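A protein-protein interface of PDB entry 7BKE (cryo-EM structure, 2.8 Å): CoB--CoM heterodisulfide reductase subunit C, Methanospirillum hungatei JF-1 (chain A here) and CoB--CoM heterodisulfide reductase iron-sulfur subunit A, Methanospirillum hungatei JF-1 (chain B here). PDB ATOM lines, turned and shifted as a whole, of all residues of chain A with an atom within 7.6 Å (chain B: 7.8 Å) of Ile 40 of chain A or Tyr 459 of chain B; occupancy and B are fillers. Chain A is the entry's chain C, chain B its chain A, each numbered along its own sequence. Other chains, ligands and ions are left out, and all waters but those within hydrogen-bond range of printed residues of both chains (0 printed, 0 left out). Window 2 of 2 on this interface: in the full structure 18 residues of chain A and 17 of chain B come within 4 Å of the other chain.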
ATOM      1  N   LEU A  34      13.102  -3.166   3.002  1.00  0.00           N
ATOM      2  CA  LEU A  34      14.082  -4.138   2.526  1.00  0.00           C
ATOM      3  C   LEU A  34      13.415  -5.465   2.196  1.00  0.00           C
ATOM      4  O   LEU A  34      13.653  -6.047   1.131  1.00  0.00           O
ATOM      5  CB  LEU A  34      15.185  -4.336   3.563  1.00  0.00           C
ATOM      6  CG  LEU A  34      16.202  -3.210   3.744  1.00  0.00           C
ATOM      7  CD1 LEU A  34      17.355  -3.677   4.597  1.00  0.00           C
ATOM      8  CD2 LEU A  34      16.702  -2.705   2.412  1.00  0.00           C
ATOM      9  N   SER A  37      11.008  -4.977  -1.007  1.00  0.00           N
ATOM     10  CA  SER A  37      11.711  -4.656  -2.238  1.00  0.00           C
ATOM     11  C   SER A  37      12.677  -5.745  -2.674  1.00  0.00           C
ATOM     12  O   SER A  37      12.988  -5.823  -3.866  1.00  0.00           O
ATOM     13  CB  SER A  37      12.466  -3.338  -2.080  1.00  0.00           C
ATOM     14  OG  SER A  37      13.381  -3.402  -1.006  1.00  0.00           O
ATOM     15  N   ARG A  38      13.165  -6.572  -1.746  1.00  0.00           N
ATOM     16  CA  ARG A  38      14.098  -7.650  -2.077  1.00  0.00           C
ATOM     17  C   ARG A  38      15.383  -7.100  -2.687  1.00  0.00           C
ATOM     18  O   ARG A  38      15.973  -7.703  -3.583  1.00  0.00           O
ATOM     19  CB  ARG A  38      13.451  -8.671  -3.014  1.00  0.00           C
ATOM     20  CG  ARG A  38      12.314  -9.456  -2.402  1.00  0.00           C
ATOM     21  CD  ARG A  38      11.471 -10.107  -3.478  1.00  0.00           C
ATOM     22  NE  ARG A  38      12.291 -10.853  -4.420  1.00  0.00           N
ATOM     23  CZ  ARG A  38      12.433 -10.530  -5.699  1.00  0.00           C
ATOM     24  NH1 ARG A  38      11.803  -9.472  -6.187  1.00  0.00           N
ATOM     25  NH2 ARG A  38      13.204 -11.260  -6.491  1.00  0.00           N
ATOM     26  N   THR A  39      15.815  -5.940  -2.205  1.00  0.00           N
ATOM     27  CA  THR A  39      17.000  -5.277  -2.724  1.00  0.00           C
ATOM     28  C   THR A  39      17.835  -4.782  -1.552  1.00  0.00           C
ATOM     29  O   THR A  39      17.348  -4.641  -0.430  1.00  0.00           O
ATOM     30  CB  THR A  39      16.628  -4.120  -3.665  1.00  0.00           C
ATOM     31  OG1 THR A  39      17.771  -3.731  -4.432  1.00  0.00           O
ATOM     32  CG2 THR A  39      16.131  -2.930  -2.879  1.00  0.00           C
ATOM     33  N   ILE A  40      19.118  -4.552  -1.819  1.00  0.00           N
ATOM     34  CA  ILE A  40      20.046  -4.060  -0.789  1.00  0.00           C
ATOM     35  C   ILE A  40      19.998  -2.537  -0.854  1.00  0.00           C
ATOM     36  O   ILE A  40      20.853  -1.866  -1.433  1.00  0.00           O
ATOM     37  CB  ILE A  40      21.455  -4.636  -0.966  1.00  0.00           C
ATOM     38  CG1 ILE A  40      21.963  -4.412  -2.392  1.00  0.00           C
ATOM     39  CG2 ILE A  40      21.480  -6.105  -0.605  1.00  0.00           C
ATOM     40  CD1 ILE A  40      23.412  -4.726  -2.580  1.00  0.00           C
ATOM     41  N   ALA A  41      18.981  -1.972  -0.206  1.00  0.00           N
ATOM     42  CA  ALA A  41      18.768  -0.535  -0.288  1.00  0.00           C
ATOM     43  C   ALA A  41      19.607   0.227   0.721  1.00  0.00           C
ATOM     44  O   ALA A  41      19.948   1.388   0.486  1.00  0.00           O
ATOM     45  CB  ALA A  41      17.294  -0.205  -0.085  1.00  0.00           C
ATOM     46  N   ASN A  42      19.950  -0.402   1.837  1.00  0.00           N
ATOM     47  CA  ASN A  42      20.770   0.237   2.855  1.00  0.00           C
ATOM     48  C   ASN A  42      22.206   0.452   2.414  1.00  0.00           C
ATOM     49  O   ASN A  42      22.985   1.006   3.191  1.00  0.00           O
ATOM     50  CB  ASN A  42      20.751  -0.595   4.130  1.00  0.00           C
ATOM     51  CG  ASN A  42      21.196  -2.018   3.892  1.00  0.00           C
ATOM     52  OD1 ASN A  42      20.591  -2.742   3.109  1.00  0.00           O
ATOM     53  ND2 ASN A  42      22.261  -2.428   4.571  1.00  0.00           N
ATOM     54  N   MET A  43      22.581   0.038   1.211  1.00  0.00           N
ATOM     55  CA  MET A  43      23.957   0.124   0.753  1.00  0.00           C
ATOM     56  C   MET A  43      24.172   1.266  -0.223  1.00  0.00           C
ATOM     57  O   MET A  43      25.214   1.322  -0.874  1.00  0.00           O
ATOM     58  CB  MET A  43      24.379  -1.199   0.116  1.00  0.00           C
ATOM     59  CG  MET A  43      24.505  -2.319   1.122  1.00  0.00           C
ATOM     60  SD  MET A  43      25.802  -2.139   2.351  1.00  0.00           S
ATOM     61  CE  MET A  43      27.133  -1.448   1.391  1.00  0.00           C
ATOM     62  N   CYS A  44      23.204   2.161  -0.353  1.00  0.00           N
ATOM     63  CA  CYS A  44      23.351   3.319  -1.218  1.00  0.00           C
ATOM     64  C   CYS A  44      24.405   4.262  -0.658  1.00  0.00           C
ATOM     65  O   CYS A  44      24.440   4.530   0.542  1.00  0.00           O
ATOM     66  CB  CYS A  44      22.005   4.035  -1.345  1.00  0.00           C
ATOM     67  SG  CYS A  44      21.987   5.562  -2.262  1.00  0.00           S
ATOM     68  N   TYR A  45      25.279   4.758  -1.525  1.00  0.00           N
ATOM     69  CA  TYR A  45      26.213   5.794  -1.110  1.00  0.00           C
ATOM     70  C   TYR A  45      26.033   7.077  -1.909  1.00  0.00           C
ATOM     71  O   TYR A  45      26.971   7.853  -2.067  1.00  0.00           O
ATOM     72  CB  TYR A  45      27.662   5.312  -1.160  1.00  0.00           C
ATOM     73  CG  TYR A  45      28.212   4.937  -2.505  1.00  0.00           C
ATOM     74  CD1 TYR A  45      28.111   3.660  -2.972  1.00  0.00           C
ATOM     75  CD2 TYR A  45      28.846   5.854  -3.300  1.00  0.00           C
ATOM     76  CE1 TYR A  45      28.628   3.303  -4.190  1.00  0.00           C
ATOM     77  CE2 TYR A  45      29.349   5.498  -4.520  1.00  0.00           C
ATOM     78  CZ  TYR A  45      29.235   4.222  -4.962  1.00  0.00           C
ATOM     79  OH  TYR A  45      29.747   3.865  -6.182  1.00  0.00           O
ATOM     80  N   MET A  68      15.852   7.242  -1.804  1.00  0.00           N
ATOM     81  CA  MET A  68      16.768   6.242  -1.264  1.00  0.00           C
ATOM     82  C   MET A  68      17.345   6.688   0.073  1.00  0.00           C
ATOM     83  O   MET A  68      17.480   5.885   1.003  1.00  0.00           O
ATOM     84  CB  MET A  68      17.897   5.965  -2.256  1.00  0.00           C
ATOM     85  CG  MET A  68      17.446   5.368  -3.572  1.00  0.00           C
ATOM     86  SD  MET A  68      16.677   3.752  -3.421  1.00  0.00           S
ATOM     87  CE  MET A  68      17.805   2.927  -2.311  1.00  0.00           C
ATOM     88  N   VAL A  72      17.005   4.895   3.726  1.00  0.00           N
ATOM     89  CA  VAL A  72      18.141   4.544   4.573  1.00  0.00           C
ATOM     90  C   VAL A  72      17.974   5.126   5.971  1.00  0.00           C
ATOM     91  O   VAL A  72      18.210   4.444   6.974  1.00  0.00           O
ATOM     92  CB  VAL A  72      19.455   5.006   3.919  1.00  0.00           C
ATOM     93  CG1 VAL A  72      20.561   5.076   4.947  1.00  0.00           C
ATOM     94  CG2 VAL A  72      19.834   4.071   2.797  1.00  0.00           C
ATOM     95  N   CYS A  98      22.782   1.588 -11.399  1.00  0.00           N
ATOM     96  CA  CYS A  98      23.306   1.790 -10.055  1.00  0.00           C
ATOM     97  C   CYS A  98      24.612   1.024  -9.863  1.00  0.00           C
ATOM     98  O   CYS A  98      24.677  -0.167 -10.180  1.00  0.00           O
ATOM     99  CB  CYS A  98      22.292   1.356  -9.003  1.00  0.00           C
ATOM    100  SG  CYS A  98      22.923   1.372  -7.329  1.00  0.00           S
ATOM    101  N   PRO A  99      25.668   1.665  -9.356  1.00  0.00           N
ATOM    102  CA  PRO A  99      26.942   0.963  -9.162  1.00  0.00           C
ATOM    103  C   PRO A  99      26.951   0.022  -7.979  1.00  0.00           C
ATOM    104  O   PRO A  99      27.913  -0.732  -7.827  1.00  0.00           O
ATOM    105  CB  PRO A  99      27.944   2.101  -8.947  1.00  0.00           C
ATOM    106  CG  PRO A  99      27.188   3.358  -9.143  1.00  0.00           C
ATOM    107  CD  PRO A  99      25.762   3.073  -8.962  1.00  0.00           C
ATOM    108  N   ARG A 100      25.936   0.054  -7.131  1.00  0.00           N
ATOM    109  CA  ARG A 100      25.877  -0.778  -5.945  1.00  0.00           C
ATOM    110  C   ARG A 100      24.935  -1.963  -6.092  1.00  0.00           C
ATOM    111  O   ARG A 100      24.704  -2.670  -5.113  1.00  0.00           O
ATOM    112  CB  ARG A 100      25.458   0.071  -4.750  1.00  0.00           C
ATOM    113  CG  ARG A 100      26.599   0.756  -4.064  1.00  0.00           C
ATOM    114  CD  ARG A 100      27.206  -0.119  -3.009  1.00  0.00           C
ATOM    115  NE  ARG A 100      28.527   0.333  -2.596  1.00  0.00           N
ATOM    116  CZ  ARG A 100      28.793   0.903  -1.429  1.00  0.00           C
ATOM    117  NH1 ARG A 100      27.825   1.119  -0.559  1.00  0.00           N
ATOM    118  NH2 ARG A 100      30.025   1.274  -1.142  1.00  0.00           N
ATOM    119  N   ASP A 101      24.395  -2.196  -7.289  1.00  0.00           N
ATOM    120  CA  ASP A 101      23.356  -3.205  -7.521  1.00  0.00           C
ATOM    121  C   ASP A 101      22.161  -3.018  -6.598  1.00  0.00           C
ATOM    122  O   ASP A 101      21.714  -3.944  -5.921  1.00  0.00           O
ATOM    123  CB  ASP A 101      23.892  -4.629  -7.398  1.00  0.00           C
ATOM    124  CG  ASP A 101      24.819  -4.996  -8.510  1.00  0.00           C
ATOM    125  OD1 ASP A 101      24.664  -4.452  -9.619  1.00  0.00           O
ATOM    126  OD2 ASP A 101      25.664  -5.881  -8.292  1.00  0.00           O
ATOM    127  N   ILE A 102      21.635  -1.812  -6.582  1.00  0.00           N
ATOM    128  CA  ILE A 102      20.394  -1.521  -5.889  1.00  0.00           C
ATOM    129  C   ILE A 102      19.308  -1.394  -6.942  1.00  0.00           C
ATOM    130  O   ILE A 102      19.576  -1.053  -8.097  1.00  0.00           O
ATOM    131  CB  ILE A 102      20.509  -0.248  -5.032  1.00  0.00           C
ATOM    132  CG1 ILE A 102      21.725  -0.357  -4.123  1.00  0.00           C
ATOM    133  CG2 ILE A 102      19.266  -0.026  -4.210  1.00  0.00           C
ATOM    134  CD1 ILE A 102      21.881   0.789  -3.204  1.00  0.00           C
ATOM    135  N   ALA A 103      18.079  -1.713  -6.548  1.00  0.00           N
ATOM    136  CA  ALA A 103      16.904  -1.499  -7.383  1.00  0.00           C
ATOM    137  C   ALA A 103      16.087  -0.376  -6.761  1.00  0.00           C
ATOM    138  O   ALA A 103      15.161  -0.627  -5.970  1.00  0.00           O
ATOM    139  CB  ALA A 103      16.078  -2.778  -7.514  1.00  0.00           C
ATOM    140  N   VAL A 107      12.505  -0.268  -4.574  1.00  0.00           N
ATOM    141  CA  VAL A 107      12.261   0.459  -3.330  1.00  0.00           C
ATOM    142  C   VAL A 107      11.038   1.359  -3.467  1.00  0.00           C
ATOM    143  O   VAL A 107      10.216   1.464  -2.551  1.00  0.00           O
ATOM    144  CB  VAL A 107      13.514   1.254  -2.927  1.00  0.00           C
ATOM    145  CG1 VAL A 107      13.164   2.358  -1.955  1.00  0.00           C
ATOM    146  CG2 VAL A 107      14.534   0.331  -2.321  1.00  0.00           C
ATOM    147  N   LEU B 425      36.300   4.257  10.541  1.00  0.00           N
ATOM    148  CA  LEU B 425      35.543   3.076  10.138  1.00  0.00           C
ATOM    149  C   LEU B 425      35.817   1.904  11.072  1.00  0.00           C
ATOM    150  O   LEU B 425      34.891   1.199  11.492  1.00  0.00           O
ATOM    151  CB  LEU B 425      35.884   2.698   8.703  1.00  0.00           C
ATOM    152  CG  LEU B 425      35.381   3.636   7.615  1.00  0.00           C
ATOM    153  CD1 LEU B 425      35.974   3.266   6.279  1.00  0.00           C
ATOM    154  CD2 LEU B 425      33.886   3.587   7.562  1.00  0.00           C
ATOM    155  N   SER B 449      38.968   5.832   1.405  1.00  0.00           N
ATOM    156  CA  SER B 449      39.388   4.445   1.545  1.00  0.00           C
ATOM    157  C   SER B 449      40.048   4.048   0.229  1.00  0.00           C
ATOM    158  O   SER B 449      39.428   3.472  -0.660  1.00  0.00           O
ATOM    159  CB  SER B 449      38.208   3.565   1.883  1.00  0.00           C
ATOM    160  OG  SER B 449      37.203   3.669   0.900  1.00  0.00           O
ATOM    161  N   MET B 453      42.094  -3.252  -0.150  1.00  0.00           N
ATOM    162  CA  MET B 453      40.960  -3.759   0.618  1.00  0.00           C
ATOM    163  C   MET B 453      40.250  -2.674   1.421  1.00  0.00           C
ATOM    164  O   MET B 453      39.353  -2.986   2.214  1.00  0.00           O
ATOM    165  CB  MET B 453      41.364  -4.900   1.563  1.00  0.00           C
ATOM    166  CG  MET B 453      42.137  -6.043   0.910  1.00  0.00           C
ATOM    167  SD  MET B 453      41.480  -6.769  -0.608  1.00  0.00           S
ATOM    168  CE  MET B 453      39.726  -6.856  -0.269  1.00  0.00           C
ATOM    169  N   TYR B 454      40.608  -1.405   1.225  1.00  0.00           N
ATOM    170  CA  TYR B 454      39.995  -0.333   2.001  1.00  0.00           C
ATOM    171  C   TYR B 454      38.557  -0.092   1.574  1.00  0.00           C
ATOM    172  O   TYR B 454      37.680   0.108   2.418  1.00  0.00           O
ATOM    173  CB  TYR B 454      40.797   0.954   1.854  1.00  0.00           C
ATOM    174  CG  TYR B 454      42.102   0.998   2.608  1.00  0.00           C
ATOM    175  CD1 TYR B 454      42.724  -0.158   3.033  1.00  0.00           C
ATOM    176  CD2 TYR B 454      42.717   2.207   2.880  1.00  0.00           C
ATOM    177  CE1 TYR B 454      43.912  -0.113   3.708  1.00  0.00           C
ATOM    178  CE2 TYR B 454      43.903   2.260   3.553  1.00  0.00           C
ATOM    179  CZ  TYR B 454      44.495   1.097   3.964  1.00  0.00           C
ATOM    180  OH  TYR B 454      45.687   1.153   4.635  1.00  0.00           O
ATOM    181  N   GLU B 455      38.304  -0.075   0.268  1.00  0.00           N
ATOM    182  CA  GLU B 455      36.946   0.124  -0.220  1.00  0.00           C
ATOM    183  C   GLU B 455      36.041  -1.017   0.219  1.00  0.00           C
ATOM    184  O   GLU B 455      34.876  -0.800   0.568  1.00  0.00           O
ATOM    185  CB  GLU B 455      36.955   0.262  -1.735  1.00  0.00           C
ATOM    186  CG  GLU B 455      35.648   0.718  -2.324  1.00  0.00           C
ATOM    187  CD  GLU B 455      35.331   2.158  -1.992  1.00  0.00           C
ATOM    188  OE1 GLU B 455      36.281   2.950  -1.838  1.00  0.00           O
ATOM    189  OE2 GLU B 455      34.136   2.497  -1.880  1.00  0.00           O
ATOM    190  N   GLU B 456      36.563  -2.239   0.215  1.00  0.00           N
ATOM    191  CA  GLU B 456      35.801  -3.375   0.716  1.00  0.00           C
ATOM    192  C   GLU B 456      35.529  -3.247   2.207  1.00  0.00           C
ATOM    193  O   GLU B 456      34.450  -3.618   2.680  1.00  0.00           O
ATOM    194  CB  GLU B 456      36.548  -4.668   0.405  1.00  0.00           C
ATOM    195  CG  GLU B 456      36.552  -5.026  -1.069  1.00  0.00           C
ATOM    196  CD  GLU B 456      37.595  -4.268  -1.876  1.00  0.00           C
ATOM    197  OE1 GLU B 456      38.203  -3.316  -1.347  1.00  0.00           O
ATOM    198  OE2 GLU B 456      37.813  -4.633  -3.046  1.00  0.00           O
ATOM    199  N   PHE B 457      36.491  -2.722   2.964  1.00  0.00           N
ATOM    200  CA  PHE B 457      36.256  -2.454   4.377  1.00  0.00           C
ATOM    201  C   PHE B 457      35.135  -1.438   4.566  1.00  0.00           C
ATOM    202  O   PHE B 457      34.281  -1.591   5.447  1.00  0.00           O
ATOM    203  CB  PHE B 457      37.550  -1.959   5.013  1.00  0.00           C
ATOM    204  CG  PHE B 457      37.513  -1.893   6.497  1.00  0.00           C
ATOM    205  CD1 PHE B 457      37.401  -3.037   7.246  1.00  0.00           C
ATOM    206  CD2 PHE B 457      37.607  -0.682   7.144  1.00  0.00           C
ATOM    207  CE1 PHE B 457      37.371  -2.973   8.606  1.00  0.00           C
ATOM    208  CE2 PHE B 457      37.584  -0.616   8.501  1.00  0.00           C
ATOM    209  CZ  PHE B 457      37.464  -1.760   9.236  1.00  0.00           C
ATOM    210  N   TYR B 458      35.136  -0.389   3.750  1.00  0.00           N
ATOM    211  CA  TYR B 458      34.095   0.633   3.797  1.00  0.00           C
ATOM    212  C   TYR B 458      32.726   0.038   3.486  1.00  0.00           C
ATOM    213  O   TYR B 458      31.732   0.320   4.173  1.00  0.00           O
ATOM    214  CB  TYR B 458      34.470   1.733   2.807  1.00  0.00           C
ATOM    215  CG  TYR B 458      33.438   2.786   2.523  1.00  0.00           C
ATOM    216  CD1 TYR B 458      32.639   3.302   3.527  1.00  0.00           C
ATOM    217  CD2 TYR B 458      33.293   3.297   1.246  1.00  0.00           C
ATOM    218  CE1 TYR B 458      31.708   4.269   3.261  1.00  0.00           C
ATOM    219  CE2 TYR B 458      32.369   4.268   0.971  1.00  0.00           C
ATOM    220  CZ  TYR B 458      31.577   4.752   1.983  1.00  0.00           C
ATOM    221  OH  TYR B 458      30.649   5.721   1.705  1.00  0.00           O
ATOM    222  N   TYR B 459      32.665  -0.799   2.456  1.00  0.00           N
ATOM    223  CA  TYR B 459      31.433  -1.496   2.112  1.00  0.00           C
ATOM    224  C   TYR B 459      30.949  -2.354   3.268  1.00  0.00           C
ATOM    225  O   TYR B 459      29.757  -2.364   3.592  1.00  0.00           O
ATOM    226  CB  TYR B 459      31.675  -2.347   0.868  1.00  0.00           C
ATOM    227  CG  TYR B 459      30.442  -2.957   0.257  1.00  0.00           C
ATOM    228  CD1 TYR B 459      29.872  -2.410  -0.875  1.00  0.00           C
ATOM    229  CD2 TYR B 459      29.862  -4.089   0.799  1.00  0.00           C
ATOM    230  CE1 TYR B 459      28.760  -2.957  -1.442  1.00  0.00           C
ATOM    231  CE2 TYR B 459      28.744  -4.641   0.243  1.00  0.00           C
ATOM    232  CZ  TYR B 459      28.198  -4.074  -0.879  1.00  0.00           C
ATOM    233  OH  TYR B 459      27.080  -4.627  -1.445  1.00  0.00           O
ATOM    234  N   ARG B 460      31.861  -3.072   3.915  1.00  0.00           N
ATOM    235  CA  ARG B 460      31.472  -3.951   5.007  1.00  0.00           C
ATOM    236  C   ARG B 460      30.966  -3.165   6.208  1.00  0.00           C
ATOM    237  O   ARG B 460      30.029  -3.595   6.889  1.00  0.00           O
ATOM    238  CB  ARG B 460      32.649  -4.838   5.393  1.00  0.00           C
ATOM    239  CG  ARG B 460      32.427  -5.648   6.642  1.00  0.00           C
ATOM    240  CD  ARG B 460      33.739  -6.136   7.187  1.00  0.00           C
ATOM    241  NE  ARG B 460      33.567  -6.938   8.388  1.00  0.00           N
ATOM    242  CZ  ARG B 460      34.573  -7.408   9.110  1.00  0.00           C
ATOM    243  NH1 ARG B 460      35.821  -7.151   8.747  1.00  0.00           N
ATOM    244  NH2 ARG B 460      34.334  -8.137  10.191  1.00  0.00           N
ATOM    245  N   ILE B 461      31.571  -2.011   6.494  1.00  0.00           N
ATOM    246  CA  ILE B 461      31.106  -1.205   7.621  1.00  0.00           C
ATOM    247  C   ILE B 461      29.712  -0.662   7.348  1.00  0.00           C
ATOM    248  O   ILE B 461      28.826  -0.707   8.215  1.00  0.00           O
ATOM    249  CB  ILE B 461      32.101  -0.073   7.935  1.00  0.00           C
ATOM    250  CG1 ILE B 461      33.471  -0.635   8.299  1.00  0.00           C
ATOM    251  CG2 ILE B 461      31.588   0.775   9.077  1.00  0.00           C
ATOM    252  CD1 ILE B 461      33.427  -1.865   9.154  1.00  0.00           C
ATOM    253  N   GLN B 462      29.488  -0.144   6.138  1.00  0.00           N
ATOM    254  CA  GLN B 462      28.141   0.304   5.803  1.00  0.00           C
ATOM    255  C   GLN B 462      27.144  -0.843   5.879  1.00  0.00           C
ATOM    256  O   GLN B 462      26.012  -0.649   6.332  1.00  0.00           O
ATOM    257  CB  GLN B 462      28.111   0.936   4.418  1.00  0.00           C
ATOM    258  CG  GLN B 462      26.748   1.486   4.074  1.00  0.00           C
ATOM    259  CD  GLN B 462      26.757   2.385   2.869  1.00  0.00           C
ATOM    260  OE1 GLN B 462      27.794   2.620   2.260  1.00  0.00           O
ATOM    261  NE2 GLN B 462      25.595   2.902   2.519  1.00  0.00           N
ATOM    262  N   HIS B 463      27.549  -2.043   5.462  1.00  0.00           N
ATOM    263  CA  HIS B 463      26.673  -3.207   5.532  1.00  0.00           C
ATOM    264  C   HIS B 463      26.319  -3.556   6.970  1.00  0.00           C
ATOM    265  O   HIS B 463      25.169  -3.888   7.265  1.00  0.00           O
ATOM    266  CB  HIS B 463      27.343  -4.383   4.831  1.00  0.00           C
ATOM    267  CG  HIS B 463      26.525  -5.633   4.824  1.00  0.00           C
ATOM    268  ND1 HIS B 463      25.406  -5.782   4.035  1.00  0.00           N
ATOM    269  CD2 HIS B 463      26.670  -6.795   5.499  1.00  0.00           C
ATOM    270  CE1 HIS B 463      24.891  -6.982   4.232  1.00  0.00           C
ATOM    271  NE2 HIS B 463      25.640  -7.618   5.113  1.00  0.00           N
ATOM    272  N   GLU B 464      27.290  -3.498   7.876  1.00  0.00           N
ATOM    273  CA  GLU B 464      26.985  -3.736   9.281  1.00  0.00           C
ATOM    274  C   GLU B 464      26.145  -2.628   9.887  1.00  0.00           C
ATOM    275  O   GLU B 464      25.529  -2.848  10.935  1.00  0.00           O
ATOM    276  CB  GLU B 464      28.262  -3.913  10.090  1.00  0.00           C
ATOM    277  CG  GLU B 464      29.098  -5.083   9.649  1.00  0.00           C
ATOM    278  CD  GLU B 464      30.361  -5.214  10.457  1.00  0.00           C
ATOM    279  OE1 GLU B 464      31.172  -6.114  10.155  1.00  0.00           O
ATOM    280  OE2 GLU B 464      30.538  -4.417  11.402  1.00  0.00           O
ATOM    281  N   GLY B 465      26.112  -1.449   9.278  1.00  0.00           N
ATOM    282  CA  GLY B 465      25.056  -0.514   9.611  1.00  0.00           C
ATOM    283  C   GLY B 465      25.476   0.784  10.257  1.00  0.00           C
ATOM    284  O   GLY B 465      24.714   1.370  11.028  1.00  0.00           O
ATOM    285  N   PHE B 468      26.271   7.096   7.669  1.00  0.00           N
ATOM    286  CA  PHE B 468      27.211   8.036   7.086  1.00  0.00           C
ATOM    287  C   PHE B 468      26.462   9.312   6.737  1.00  0.00           C
ATOM    288  O   PHE B 468      25.643   9.324   5.816  1.00  0.00           O
ATOM    289  CB  PHE B 468      27.892   7.439   5.860  1.00  0.00           C
ATOM    290  CG  PHE B 468      28.806   6.301   6.180  1.00  0.00           C
ATOM    291  CD1 PHE B 468      30.156   6.508   6.342  1.00  0.00           C
ATOM    292  CD2 PHE B 468      28.308   5.023   6.322  1.00  0.00           C
ATOM    293  CE1 PHE B 468      30.988   5.463   6.634  1.00  0.00           C
ATOM    294  CE2 PHE B 468      29.136   3.979   6.615  1.00  0.00           C
ATOM    295  CZ  PHE B 468      30.473   4.193   6.773  1.00  0.00           C
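O of Asn 42 of chain A sits at hydrogen-bond distance from NE2 of Gln 462 of chain B (3.3 Å).
The backbone carbonyl oxygen (O) of Cys 44 of chain A is in hydrogen-bond range of the side-chain amide nitrogen (NE2) of Gln 462 of chain B (2.8 Å).
The guanidinium group (NH1) of Arg 100 of chain A lies within hydrogen-bond range of the side-chain amide oxygen (OE1) of Gln 462 of chain B, at 3.2 Å.
The side-chain sulfur of Met 43 of chain A sits close to the backbone NH of His 463 of chain B (3.6 Å).
The side-chain sulfur (SG) of Cys 98 of chain A sits close to the backbone NH (N) of Arg 100 of chain A, at 3.3 Å.
The backbone carbonyl oxygen (O) of Met 43 of chain A is in hydrogen-bond range of the guanidinium group (NH1) of Arg 100 of chain A (2.6 Å).
Ile 40 of chain A touches Tyr 459 of chain B (CD1 to OH, 3.8 Å).
Tyr 459 of chain B touches Met 43 of chain A (O to CE, 3.5 Å).
Met 43 of chain A touches Gln 462 of chain B (C to NE2, 3.5 Å).
Arg 100 of chain A touches Tyr 459 of chain B (NE to CE1, 3.5 Å).
Ile 40 of chain A touches one residue of chain B.
Of chain A, only Ile 40 (3.8 Å), Met 43 (3.5 Å) and Arg 100 (3.5 Å) come within 4 Å of Tyr 459 of chain B.
Of the printed residues of chain B, Asn 42 of chain A touches Gln 462.
Of the printed residues of chain B, Cys 44 of chain A touches Gln 462.
Of the printed residues of chain A, Gln 462 of chain B touches Asn 42 (3.3 Å), Met 43 (3.5 Å), Cys 44 (2.8 Å) and Arg 100 (3.2 Å).
Printed residues of chain B within 4 Å of Met 43 of chain A: Tyr 459 (3.5 Å), Gln 462 (3.5 Å) and His 463 (3.5 Å).
Ser 449 of chain B touches none of the printed residues of chain A.
Val 107 of chain A touches none of the printed residues of chain B.
The nearest printed residue of chain B that does not touch Cys 44 of chain A is Tyr 458 of chain B (6.4 Å).
Of the 19 printed residues of chain A, 5 touch a printed residue of chain B.
Printed residues of chain A that touch a printed residue of chain B: Ile 40, Asn 42, Met 43, Cys 44 and Arg 100.
Hydrophobic or aromatic side chains of chain A within 4 Å of the printed part of chain B: Ile 40 and Met 43.
Hydrophobic or aromatic side chains of chain B within 4 Å of the printed part of chain A: Tyr 459 and His 463.
Among the printed residues, 8 pairs touch across the chains.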
